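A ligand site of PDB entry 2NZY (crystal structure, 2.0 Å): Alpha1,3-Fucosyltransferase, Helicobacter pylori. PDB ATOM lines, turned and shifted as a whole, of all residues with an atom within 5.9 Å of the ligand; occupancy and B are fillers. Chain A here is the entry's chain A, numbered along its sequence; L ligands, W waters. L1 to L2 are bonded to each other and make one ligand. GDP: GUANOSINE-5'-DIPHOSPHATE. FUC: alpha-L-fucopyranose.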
ATOM      1  N   GLY A  94     -15.660   6.130  13.326  1.00  0.00           N
ATOM      2  CA  GLY A  94     -14.884   5.855  12.140  1.00  0.00           C
ATOM      3  C   GLY A  94     -15.390   6.697  10.958  1.00  0.00           C
ATOM      4  O   GLY A  94     -14.647   6.983  10.024  1.00  0.00           O
ATOM      5  N   GLU A  95     -16.652   7.123  11.051  1.00  0.00           N
ATOM      6  CA  GLU A  95     -17.293   7.936  10.041  1.00  0.00           C
ATOM      7  C   GLU A  95     -16.729   9.351   9.850  1.00  0.00           C
ATOM      8  O   GLU A  95     -15.973   9.872  10.659  1.00  0.00           O
ATOM      9  CB  GLU A  95     -18.769   8.085  10.385  1.00  0.00           C
ATOM     10  CG  GLU A  95     -19.463   6.855  10.842  1.00  0.00           C
ATOM     11  CD  GLU A  95     -19.568   5.865   9.715  1.00  0.00           C
ATOM     12  OE1 GLU A  95     -20.250   6.183   8.706  1.00  0.00           O
ATOM     13  OE2 GLU A  95     -18.954   4.790   9.827  1.00  0.00           O
ATOM     14  N   ASN A  96     -17.174   9.971   8.782  1.00  0.00           N
ATOM     15  CA  ASN A  96     -16.816  11.348   8.423  1.00  0.00           C
ATOM     16  C   ASN A  96     -17.956  12.200   9.050  1.00  0.00           C
ATOM     17  O   ASN A  96     -18.871  12.645   8.388  1.00  0.00           O
ATOM     18  CB  ASN A  96     -16.801  11.470   6.904  1.00  0.00           C
ATOM     19  CG  ASN A  96     -16.654  12.883   6.457  1.00  0.00           C
ATOM     20  OD1 ASN A  96     -16.237  13.736   7.226  1.00  0.00           O
ATOM     21  ND2 ASN A  96     -16.965  13.141   5.182  1.00  0.00           N
ATOM     22  N   LEU A 124      -7.964   8.056  11.348  1.00  0.00           N
ATOM     23  CA  LEU A 124      -8.024   6.613  11.209  1.00  0.00           C
ATOM     24  C   LEU A 124      -6.666   6.046  10.634  1.00  0.00           C
ATOM     25  O   LEU A 124      -6.261   4.880  10.918  1.00  0.00           O
ATOM     26  CB  LEU A 124      -9.167   6.348  10.289  1.00  0.00           C
ATOM     27  CG  LEU A 124      -9.966   5.094  10.377  1.00  0.00           C
ATOM     28  CD1 LEU A 124     -10.443   4.837  11.787  1.00  0.00           C
ATOM     29  CD2 LEU A 124     -11.141   5.297   9.390  1.00  0.00           C
ATOM     30  N   ARG A 128      -4.471   2.424  11.422  1.00  0.00           N
ATOM     31  CA  ARG A 128      -4.141   1.482  10.367  1.00  0.00           C
ATOM     32  C   ARG A 128      -2.654   1.192  10.491  1.00  0.00           C
ATOM     33  O   ARG A 128      -2.276   0.044  10.380  1.00  0.00           O
ATOM     34  CB  ARG A 128      -4.436   2.062   8.981  1.00  0.00           C
ATOM     35  CG  ARG A 128      -4.272   1.015   7.838  1.00  0.00           C
ATOM     36  CD  ARG A 128      -5.055  -0.226   8.165  1.00  0.00           C
ATOM     37  NE  ARG A 128      -5.569  -0.836   6.938  1.00  0.00           N
ATOM     38  CZ  ARG A 128      -6.571  -1.706   6.875  1.00  0.00           C
ATOM     39  NH1 ARG A 128      -7.195  -2.117   7.979  1.00  0.00           N
ATOM     40  NH2 ARG A 128      -7.004  -2.114   5.699  1.00  0.00           N
ATOM     41  N   VAL A 186     -10.010  -1.231  -4.911  1.00  0.00           N
ATOM     42  CA  VAL A 186     -10.746  -2.145  -4.052  1.00  0.00           C
ATOM     43  C   VAL A 186     -11.759  -1.360  -3.206  1.00  0.00           C
ATOM     44  O   VAL A 186     -11.388  -0.653  -2.257  1.00  0.00           O
ATOM     45  CB  VAL A 186      -9.833  -2.944  -3.098  1.00  0.00           C
ATOM     46  CG1 VAL A 186     -10.656  -4.024  -2.439  1.00  0.00           C
ATOM     47  CG2 VAL A 186      -8.647  -3.497  -3.811  1.00  0.00           C
ATOM     48  N   ALA A 187     -13.039  -1.495  -3.551  1.00  0.00           N
ATOM     49  CA  ALA A 187     -14.127  -0.809  -2.839  1.00  0.00           C
ATOM     50  C   ALA A 187     -15.403  -1.639  -2.863  1.00  0.00           C
ATOM     51  O   ALA A 187     -15.748  -2.214  -3.906  1.00  0.00           O
ATOM     52  CB  ALA A 187     -14.377   0.545  -3.473  1.00  0.00           C
ATOM     53  N   SER A 188     -16.103  -1.738  -1.736  1.00  0.00           N
ATOM     54  CA  SER A 188     -17.353  -2.499  -1.736  1.00  0.00           C
ATOM     55  C   SER A 188     -18.574  -1.688  -1.332  1.00  0.00           C
ATOM     56  O   SER A 188     -19.703  -2.149  -1.456  1.00  0.00           O
ATOM     57  CB  SER A 188     -17.198  -3.751  -0.886  1.00  0.00           C
ATOM     58  OG  SER A 188     -16.281  -4.602  -1.554  1.00  0.00           O
ATOM     59  N   ASN A 189     -18.346  -0.468  -0.878  1.00  0.00           N
ATOM     60  CA  ASN A 189     -19.441   0.427  -0.518  1.00  0.00           C
ATOM     61  C   ASN A 189     -19.887   1.072  -1.838  1.00  0.00           C
ATOM     62  O   ASN A 189     -19.153   1.846  -2.429  1.00  0.00           O
ATOM     63  CB  ASN A 189     -18.970   1.514   0.426  1.00  0.00           C
ATOM     64  CG  ASN A 189     -20.080   2.507   0.750  1.00  0.00           C
ATOM     65  OD1 ASN A 189     -21.035   2.684  -0.037  1.00  0.00           O
ATOM     66  ND2 ASN A 189     -19.955   3.158   1.889  1.00  0.00           N
ATOM     67  N   ASN A 191     -22.230   3.355  -2.423  1.00  0.00           N
ATOM     68  CA  ASN A 191     -22.481   4.781  -2.283  1.00  0.00           C
ATOM     69  C   ASN A 191     -21.185   5.559  -2.141  1.00  0.00           C
ATOM     70  O   ASN A 191     -20.698   5.756  -1.036  1.00  0.00           O
ATOM     71  CB  ASN A 191     -23.413   5.018  -1.080  1.00  0.00           C
ATOM     72  CG  ASN A 191     -23.968   6.445  -1.024  1.00  0.00           C
ATOM     73  OD1 ASN A 191     -23.691   7.274  -1.889  1.00  0.00           O
ATOM     74  ND2 ASN A 191     -24.770   6.733   0.009  1.00  0.00           N
ATOM     75  N   ALA A 192     -20.622   5.992  -3.260  1.00  0.00           N
ATOM     76  CA  ALA A 192     -19.396   6.801  -3.255  1.00  0.00           C
ATOM     77  C   ALA A 192     -19.235   7.397  -4.656  1.00  0.00           C
ATOM     78  O   ALA A 192     -18.271   7.117  -5.381  1.00  0.00           O
ATOM     79  CB  ALA A 192     -18.184   5.957  -2.872  1.00  0.00           C
ATOM     80  N   ARG A 195     -15.772   8.702  -6.301  1.00  0.00           N
ATOM     81  CA  ARG A 195     -14.842   7.606  -6.492  1.00  0.00           C
ATOM     82  C   ARG A 195     -15.304   6.743  -7.706  1.00  0.00           C
ATOM     83  O   ARG A 195     -14.518   6.446  -8.645  1.00  0.00           O
ATOM     84  CB  ARG A 195     -14.786   6.821  -5.171  1.00  0.00           C
ATOM     85  CG  ARG A 195     -14.279   5.401  -5.202  1.00  0.00           C
ATOM     86  CD  ARG A 195     -13.887   4.968  -3.811  1.00  0.00           C
ATOM     87  NE  ARG A 195     -14.930   4.209  -3.132  1.00  0.00           N
ATOM     88  CZ  ARG A 195     -15.008   4.029  -1.810  1.00  0.00           C
ATOM     89  NH1 ARG A 195     -14.088   4.572  -1.012  1.00  0.00           N
ATOM     90  NH2 ARG A 195     -15.976   3.280  -1.270  1.00  0.00           N
ATOM     91  N   GLY A 211     -10.894  -5.039  -7.521  1.00  0.00           N
ATOM     92  CA  GLY A 211     -10.880  -6.186  -6.607  1.00  0.00           C
ATOM     93  C   GLY A 211     -11.981  -6.278  -5.546  1.00  0.00           C
ATOM     94  O   GLY A 211     -12.129  -7.272  -4.826  1.00  0.00           O
ATOM     95  N   GLY A 212     -12.770  -5.217  -5.421  1.00  0.00           N
ATOM     96  CA  GLY A 212     -13.862  -5.226  -4.468  1.00  0.00           C
ATOM     97  C   GLY A 212     -15.201  -5.457  -5.182  1.00  0.00           C
ATOM     98  O   GLY A 212     -15.221  -5.753  -6.375  1.00  0.00           O
ATOM     99  N   SER A 213     -16.311  -5.326  -4.468  1.00  0.00           N
ATOM    100  CA  SER A 213     -17.633  -5.524  -5.086  1.00  0.00           C
ATOM    101  C   SER A 213     -17.984  -4.449  -6.079  1.00  0.00           C
ATOM    102  O   SER A 213     -18.832  -4.660  -6.942  1.00  0.00           O
ATOM    103  CB  SER A 213     -18.714  -5.555  -4.017  1.00  0.00           C
ATOM    104  OG  SER A 213     -18.755  -6.810  -3.383  1.00  0.00           O
ATOM    105  N   ASN A 221     -14.069 -11.245  -5.000  1.00  0.00           N
ATOM    106  CA  ASN A 221     -13.511 -10.227  -4.109  1.00  0.00           C
ATOM    107  C   ASN A 221     -12.222 -10.676  -3.433  1.00  0.00           C
ATOM    108  O   ASN A 221     -12.188 -11.676  -2.727  1.00  0.00           O
ATOM    109  CB  ASN A 221     -14.571  -9.796  -3.098  1.00  0.00           C
ATOM    110  CG  ASN A 221     -15.864  -9.389  -3.786  1.00  0.00           C
ATOM    111  OD1 ASN A 221     -15.869  -8.995  -4.957  1.00  0.00           O
ATOM    112  ND2 ASN A 221     -16.973  -9.468  -3.063  1.00  0.00           N
ATOM    113  N   VAL A 222     -11.166  -9.905  -3.681  1.00  0.00           N
ATOM    114  CA  VAL A 222      -9.840 -10.159  -3.173  1.00  0.00           C
ATOM    115  C   VAL A 222      -9.865 -10.352  -1.672  1.00  0.00           C
ATOM    116  O   VAL A 222     -10.561  -9.609  -0.962  1.00  0.00           O
ATOM    117  CB  VAL A 222      -8.900  -8.986  -3.578  1.00  0.00           C
ATOM    118  CG1 VAL A 222      -9.190  -7.747  -2.736  1.00  0.00           C
ATOM    119  CG2 VAL A 222      -7.462  -9.399  -3.465  1.00  0.00           C
ATOM    120  N   LYS A 223      -9.154 -11.345  -1.149  1.00  0.00           N
ATOM    121  CA  LYS A 223      -9.156 -11.558   0.295  1.00  0.00           C
ATOM    122  C   LYS A 223      -8.000 -10.817   0.949  1.00  0.00           C
ATOM    123  O   LYS A 223      -8.087 -10.401   2.101  1.00  0.00           O
ATOM    124  CB  LYS A 223      -9.054 -13.034   0.642  1.00  0.00           C
ATOM    125  CG  LYS A 223      -7.681 -13.634   0.343  1.00  0.00           C
ATOM    126  CD  LYS A 223      -7.557 -15.026   0.983  1.00  0.00           C
ATOM    127  CE  LYS A 223      -6.261 -15.749   0.552  1.00  0.00           C
ATOM    128  NZ  LYS A 223      -6.151 -15.932  -0.928  1.00  0.00           N
ATOM    129  N   ASN A 224      -6.909 -10.654   0.222  1.00  0.00           N
ATOM    130  CA  ASN A 224      -5.799  -9.908   0.793  1.00  0.00           C
ATOM    131  C   ASN A 224      -5.558  -8.646  -0.035  1.00  0.00           C
ATOM    132  O   ASN A 224      -4.869  -8.659  -1.096  1.00  0.00           O
ATOM    133  CB  ASN A 224      -4.526 -10.733   0.857  1.00  0.00           C
ATOM    134  CG  ASN A 224      -3.419 -10.010   1.562  1.00  0.00           C
ATOM    135  OD1 ASN A 224      -3.358  -8.758   1.567  1.00  0.00           O
ATOM    136  ND2 ASN A 224      -2.504 -10.768   2.145  1.00  0.00           N
ATOM    137  N   LYS A 225      -6.144  -7.549   0.452  1.00  0.00           N
ATOM    138  CA  LYS A 225      -6.063  -6.279  -0.228  1.00  0.00           C
ATOM    139  C   LYS A 225      -4.601  -5.855  -0.477  1.00  0.00           C
ATOM    140  O   LYS A 225      -4.227  -5.395  -1.579  1.00  0.00           O
ATOM    141  CB  LYS A 225      -6.822  -5.186   0.550  1.00  0.00           C
ATOM    142  CG  LYS A 225      -6.651  -3.759  -0.022  1.00  0.00           C
ATOM    143  CD  LYS A 225      -7.363  -2.659   0.808  1.00  0.00           C
ATOM    144  CE  LYS A 225      -7.084  -1.283   0.142  1.00  0.00           C
ATOM    145  NZ  LYS A 225      -7.392  -0.032   0.913  1.00  0.00           N
ATOM    146  N   PHE A 238      -9.575   6.480  -3.061  1.00  0.00           N
ATOM    147  CA  PHE A 238     -10.538   7.528  -2.760  1.00  0.00           C
ATOM    148  C   PHE A 238     -11.351   7.252  -1.508  1.00  0.00           C
ATOM    149  O   PHE A 238     -11.765   6.098  -1.300  1.00  0.00           O
ATOM    150  CB  PHE A 238     -11.500   7.682  -3.951  1.00  0.00           C
ATOM    151  CG  PHE A 238     -10.969   8.529  -5.059  1.00  0.00           C
ATOM    152  CD1 PHE A 238      -9.647   8.402  -5.481  1.00  0.00           C
ATOM    153  CD2 PHE A 238     -11.785   9.466  -5.681  1.00  0.00           C
ATOM    154  CE1 PHE A 238      -9.134   9.189  -6.502  1.00  0.00           C
ATOM    155  CE2 PHE A 238     -11.293  10.275  -6.707  1.00  0.00           C
ATOM    156  CZ  PHE A 238      -9.954  10.134  -7.127  1.00  0.00           C
ATOM    157  N   GLU A 239     -11.574   8.305  -0.718  1.00  0.00           N
ATOM    158  CA  GLU A 239     -12.416   8.204   0.472  1.00  0.00           C
ATOM    159  C   GLU A 239     -13.848   8.218  -0.093  1.00  0.00           C
ATOM    160  O   GLU A 239     -14.072   8.639  -1.238  1.00  0.00           O
ATOM    161  CB  GLU A 239     -12.234   9.414   1.414  1.00  0.00           C
ATOM    162  CG  GLU A 239     -10.785   9.733   1.766  1.00  0.00           C
ATOM    163  CD  GLU A 239     -10.182   8.762   2.720  1.00  0.00           C
ATOM    164  OE1 GLU A 239     -10.825   7.732   3.038  1.00  0.00           O
ATOM    165  OE2 GLU A 239      -9.056   9.032   3.166  1.00  0.00           O
ATOM    166  N   ASN A 240     -14.837   7.784   0.687  1.00  0.00           N
ATOM    167  CA  ASN A 240     -16.180   7.762   0.158  1.00  0.00           C
ATOM    168  C   ASN A 240     -16.833   9.152   0.185  1.00  0.00           C
ATOM    169  O   ASN A 240     -17.841   9.372  -0.477  1.00  0.00           O
ATOM    170  CB  ASN A 240     -17.040   6.763   0.928  1.00  0.00           C
ATOM    171  CG  ASN A 240     -17.571   7.361   2.197  1.00  0.00           C
ATOM    172  OD1 ASN A 240     -18.774   7.601   2.311  1.00  0.00           O
ATOM    173  ND2 ASN A 240     -16.682   7.644   3.137  1.00  0.00           N
ATOM    174  N   TYR A 246     -10.150  14.314   6.882  1.00  0.00           N
ATOM    175  CA  TYR A 246     -10.698  12.960   6.830  1.00  0.00           C
ATOM    176  C   TYR A 246      -9.850  12.015   5.974  1.00  0.00           C
ATOM    177  O   TYR A 246     -10.142  11.746   4.816  1.00  0.00           O
ATOM    178  CB  TYR A 246     -12.120  12.999   6.319  1.00  0.00           C
ATOM    179  CG  TYR A 246     -12.827  11.676   6.318  1.00  0.00           C
ATOM    180  CD1 TYR A 246     -12.966  10.960   7.490  1.00  0.00           C
ATOM    181  CD2 TYR A 246     -13.381  11.157   5.138  1.00  0.00           C
ATOM    182  CE1 TYR A 246     -13.642   9.755   7.509  1.00  0.00           C
ATOM    183  CE2 TYR A 246     -14.061   9.930   5.134  1.00  0.00           C
ATOM    184  CZ  TYR A 246     -14.185   9.246   6.308  1.00  0.00           C
ATOM    185  OH  TYR A 246     -14.850   8.029   6.341  1.00  0.00           O
ATOM    186  N   THR A 248      -8.446   8.279   5.887  1.00  0.00           N
ATOM    187  CA  THR A 248      -8.599   6.980   6.525  1.00  0.00           C
ATOM    188  C   THR A 248      -7.468   5.980   6.281  1.00  0.00           C
ATOM    189  O   THR A 248      -6.340   6.367   5.980  1.00  0.00           O
ATOM    190  CB  THR A 248      -9.913   6.350   6.105  1.00  0.00           C
ATOM    191  OG1 THR A 248      -9.916   6.216   4.686  1.00  0.00           O
ATOM    192  CG2 THR A 248     -11.099   7.279   6.491  1.00  0.00           C
ATOM    193  N   GLU A 249      -7.772   4.702   6.447  1.00  0.00           N
ATOM    194  CA  GLU A 249      -6.772   3.637   6.273  1.00  0.00           C
ATOM    195  C   GLU A 249      -6.327   3.505   4.814  1.00  0.00           C
ATOM    196  O   GLU A 249      -5.218   3.095   4.529  1.00  0.00           O
ATOM    197  CB  GLU A 249      -7.337   2.291   6.749  1.00  0.00           C
ATOM    198  CG  GLU A 249      -8.381   1.609   5.809  1.00  0.00           C
ATOM    199  CD  GLU A 249      -9.675   2.418   5.605  1.00  0.00           C
ATOM    200  OE1 GLU A 249     -10.076   3.195   6.538  1.00  0.00           O
ATOM    201  OE2 GLU A 249     -10.317   2.271   4.527  1.00  0.00           O
ATOM    202  N   LYS A 250      -7.177   3.883   3.879  1.00  0.00           N
ATOM    203  CA  LYS A 250      -6.862   3.756   2.487  1.00  0.00           C
ATOM    204  C   LYS A 250      -5.471   4.154   1.979  1.00  0.00           C
ATOM    205  O   LYS A 250      -4.839   3.330   1.301  1.00  0.00           O
ATOM    206  CB  LYS A 250      -7.953   4.451   1.689  1.00  0.00           C
ATOM    207  CG  LYS A 250      -9.359   3.964   2.072  1.00  0.00           C
ATOM    208  CD  LYS A 250     -10.438   4.833   1.378  1.00  0.00           C
ATOM    209  CE  LYS A 250     -11.819   4.302   1.669  1.00  0.00           C
ATOM    210  NZ  LYS A 250     -12.058   4.042   3.127  1.00  0.00           N
ATOM    211  N   ASP A 253      -2.776   1.789   3.070  1.00  0.00           N
ATOM    212  CA  ASP A 253      -2.678   0.495   2.409  1.00  0.00           C
ATOM    213  C   ASP A 253      -1.866   0.621   1.109  1.00  0.00           C
ATOM    214  O   ASP A 253      -1.147  -0.287   0.721  1.00  0.00           O
ATOM    215  CB  ASP A 253      -4.047  -0.035   2.145  1.00  0.00           C
ATOM    216  CG  ASP A 253      -4.775  -0.438   3.414  1.00  0.00           C
ATOM    217  OD1 ASP A 253      -4.113  -0.646   4.429  1.00  0.00           O
ATOM    218  OD2 ASP A 253      -6.004  -0.555   3.399  1.00  0.00           O
HETATM  219  PB  GDP L   1     -16.168   2.818   2.554  1.00  0.00           P
HETATM  220  O1B GDP L   1     -17.393   2.977   3.378  1.00  0.00           O
HETATM  221  O2B GDP L   1     -14.969   3.479   3.284  1.00  0.00           O
HETATM  222  O3B GDP L   1     -16.342   3.553   1.135  1.00  0.00           O
HETATM  223  O3A GDP L   1     -16.015   1.205   2.492  1.00  0.00           O
HETATM  224  PA  GDP L   1     -14.990   0.668   1.373  1.00  0.00           P
HETATM  225  O1A GDP L   1     -15.757   0.129   0.244  1.00  0.00           O
HETATM  226  O2A GDP L   1     -14.044   1.870   0.843  1.00  0.00           O
HETATM  227  O5' GDP L   1     -14.146  -0.511   2.035  1.00  0.00           O
HETATM  228  C5' GDP L   1     -13.434  -0.011   3.169  1.00  0.00           C
HETATM  229  C4' GDP L   1     -12.022  -0.676   3.216  1.00  0.00           C
HETATM  230  O4' GDP L   1     -12.166  -2.117   3.008  1.00  0.00           O
HETATM  231  C3' GDP L   1     -11.131  -0.150   2.085  1.00  0.00           C
HETATM  232  O3' GDP L   1      -9.792  -0.070   2.487  1.00  0.00           O
HETATM  233  C2' GDP L   1     -11.336  -1.166   0.996  1.00  0.00           C
HETATM  234  O2' GDP L   1     -10.254  -1.155   0.093  1.00  0.00           O
HETATM  235  C1' GDP L   1     -11.492  -2.471   1.782  1.00  0.00           C
HETATM  236  N9  GDP L   1     -12.255  -3.414   0.993  1.00  0.00           N
HETATM  237  C8  GDP L   1     -13.472  -3.203   0.375  1.00  0.00           C
HETATM  238  N7  GDP L   1     -13.852  -4.270  -0.253  1.00  0.00           N
HETATM  239  C5  GDP L   1     -12.911  -5.236  -0.078  1.00  0.00           C
HETATM  240  C6  GDP L   1     -12.767  -6.598  -0.538  1.00  0.00           C
HETATM  241  O6  GDP L   1     -13.638  -7.122  -1.256  1.00  0.00           O
HETATM  242  N1  GDP L   1     -11.634  -7.312  -0.139  1.00  0.00           N
HETATM  243  C2  GDP L   1     -10.666  -6.716   0.672  1.00  0.00           C
HETATM  244  N2  GDP L   1      -9.553  -7.440   1.072  1.00  0.00           N
HETATM  245  N3  GDP L   1     -10.803  -5.450   1.087  1.00  0.00           N
HETATM  246  C4  GDP L   1     -11.887  -4.691   0.742  1.00  0.00           C
HETATM  247  C1  FUC L   2     -15.017   3.415   4.687  1.00  0.00           C
HETATM  248  C2  FUC L   2     -14.766   4.830   5.348  1.00  0.00           C
HETATM  249  C3  FUC L   2     -14.687   4.690   6.879  1.00  0.00           C
HETATM  250  C4  FUC L   2     -13.612   3.646   7.170  1.00  0.00           C
HETATM  251  C5  FUC L   2     -14.059   2.304   6.561  1.00  0.00           C
HETATM  252  C6  FUC L   2     -13.132   1.147   6.882  1.00  0.00           C
HETATM  253  O2  FUC L   2     -15.849   5.701   5.048  1.00  0.00           O
HETATM  254  O3  FUC L   2     -14.356   5.952   7.465  1.00  0.00           O
HETATM  255  O4  FUC L   2     -12.414   4.061   6.530  1.00  0.00           O
HETATM  256  O5  FUC L   2     -14.094   2.432   5.129  1.00  0.00           O
HETATM  257  O   HOH W   1     -18.160   0.733   4.108  1.00  0.00           O
HETATM  258  O   HOH W   2     -16.749  -7.756   0.014  1.00  0.00           O
HETATM  259  O   HOH W   3     -13.264   6.951   3.135  1.00  0.00           O
HETATM  260  O   HOH W   4      -7.714  -7.476   2.903  1.00  0.00           O
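O of Phe 238 is in hydrogen-bond range of NH1 of Arg 195 (2.8 Å). O of Gly 211 is in hydrogen-bond range of N of Val 222, at 3.0 Å. The backbone NH (N) of Ser 213 sits at hydrogen-bond distance from the side-chain hydroxyl (OG) of Ser 188 (3.0 Å). The side-chain carboxylate (OD2) of Asp 253 is in salt-bridge range of the side-chain amino group (NZ) of Lys 225 (2.9 Å). The side-chain amide oxygen (OD1) of Asn 189 lies within hydrogen-bond range of the backbone NH (N) of Asn 191 (2.8 Å). The side-chain amino group (NZ) of Lys 250 lies within hydrogen-bond range of the side-chain hydroxyl (OG1) of Thr 248 (3.4 Å). The side-chain amide nitrogen (ND2) of Asn 221 is in hydrogen-bond range of the side-chain hydroxyl (OG) of Ser 213 (3.2 Å). The backbone carbonyl oxygen (O) of Ala 187 is in hydrogen-bond range of the backbone NH (N) of Ser 213.
The side-chain hydroxyl (OH) of Tyr 246 is in hydrogen-bond range of an oxygen (O3) of FUC L2 (2.4 Å). An oxygen (O3B) of GDP L1 is in salt-bridge range of the guanidinium group of Arg 195 (2.4 Å). The side-chain carboxylate (OE1) of Glu 249 is in hydrogen-bond range of an oxygen (O4) of FUC L2 (2.5 Å). The backbone carbonyl oxygen (O) of Val 186 lies within hydrogen-bond range of an oxygen (O2') of GDP L1 (2.7 Å). A nitrogen (N1) of GDP L1 is in hydrogen-bond range of the backbone carbonyl oxygen of Val 222 (2.7 Å). N of Ser 188 sits at hydrogen-bond distance from O1A of GDP L1 (2.7 Å). N7 of GDP L1 is in hydrogen-bond range of OG of Ser 188, at 2.8 Å. O of Gly 94 is in hydrogen-bond range of O3 of FUC L2 (2.8 Å). The side-chain amide nitrogen of Asn 240 lies within hydrogen-bond range of an oxygen (O2) of FUC L2. O3' of GDP L1 lies within hydrogen-bond range of NZ of Lys 225. N of Asn 189 sits at hydrogen-bond distance from O1A of GDP L1 (2.9 Å). The side-chain amide nitrogen of Asn 189 lies within hydrogen-bond range of an oxygen (O1B) of GDP L1 (3.0 Å). The side-chain amino group (NZ) of Lys 250 is in salt-bridge range of an oxygen (O2A) of GDP L1, at 3.7 Å. The backbone carbonyl oxygen of Lys 223 lies within hydrogen-bond range of a nitrogen (N2) of GDP L1.
CD2 of Leu 124 touches O4 of FUC L2 (3.4 Å). C of Ala 187 touches O1A of GDP L1, 3.6 Å away. O of Gly 211 touches O6 of GDP L1, at 3.9 Å. CA of Gly 212 touches O6 of GDP L1, at 3.7 Å. Asn 221 touches the ligand. CB of Thr 248 touches O4 of FUC L2 (3.4 Å). Asp 253 touches the ligand. The nearest printed residue that does not touch the ligand is Asn 224 (4.2 Å).
Water W4 lies within hydrogen-bond range of N2 of GDP L1 (2.6 Å), N of Lys 225 (2.9 Å) and O of Lys 223 (3.1 Å). Water W3 lies within hydrogen-bond range of OE1 of Glu 239 (2.6 Å), N of Asn 240 (3.0 Å), NZ of Lys 250 (3.1 Å) and O2 of FUC L2 (3.5 Å).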
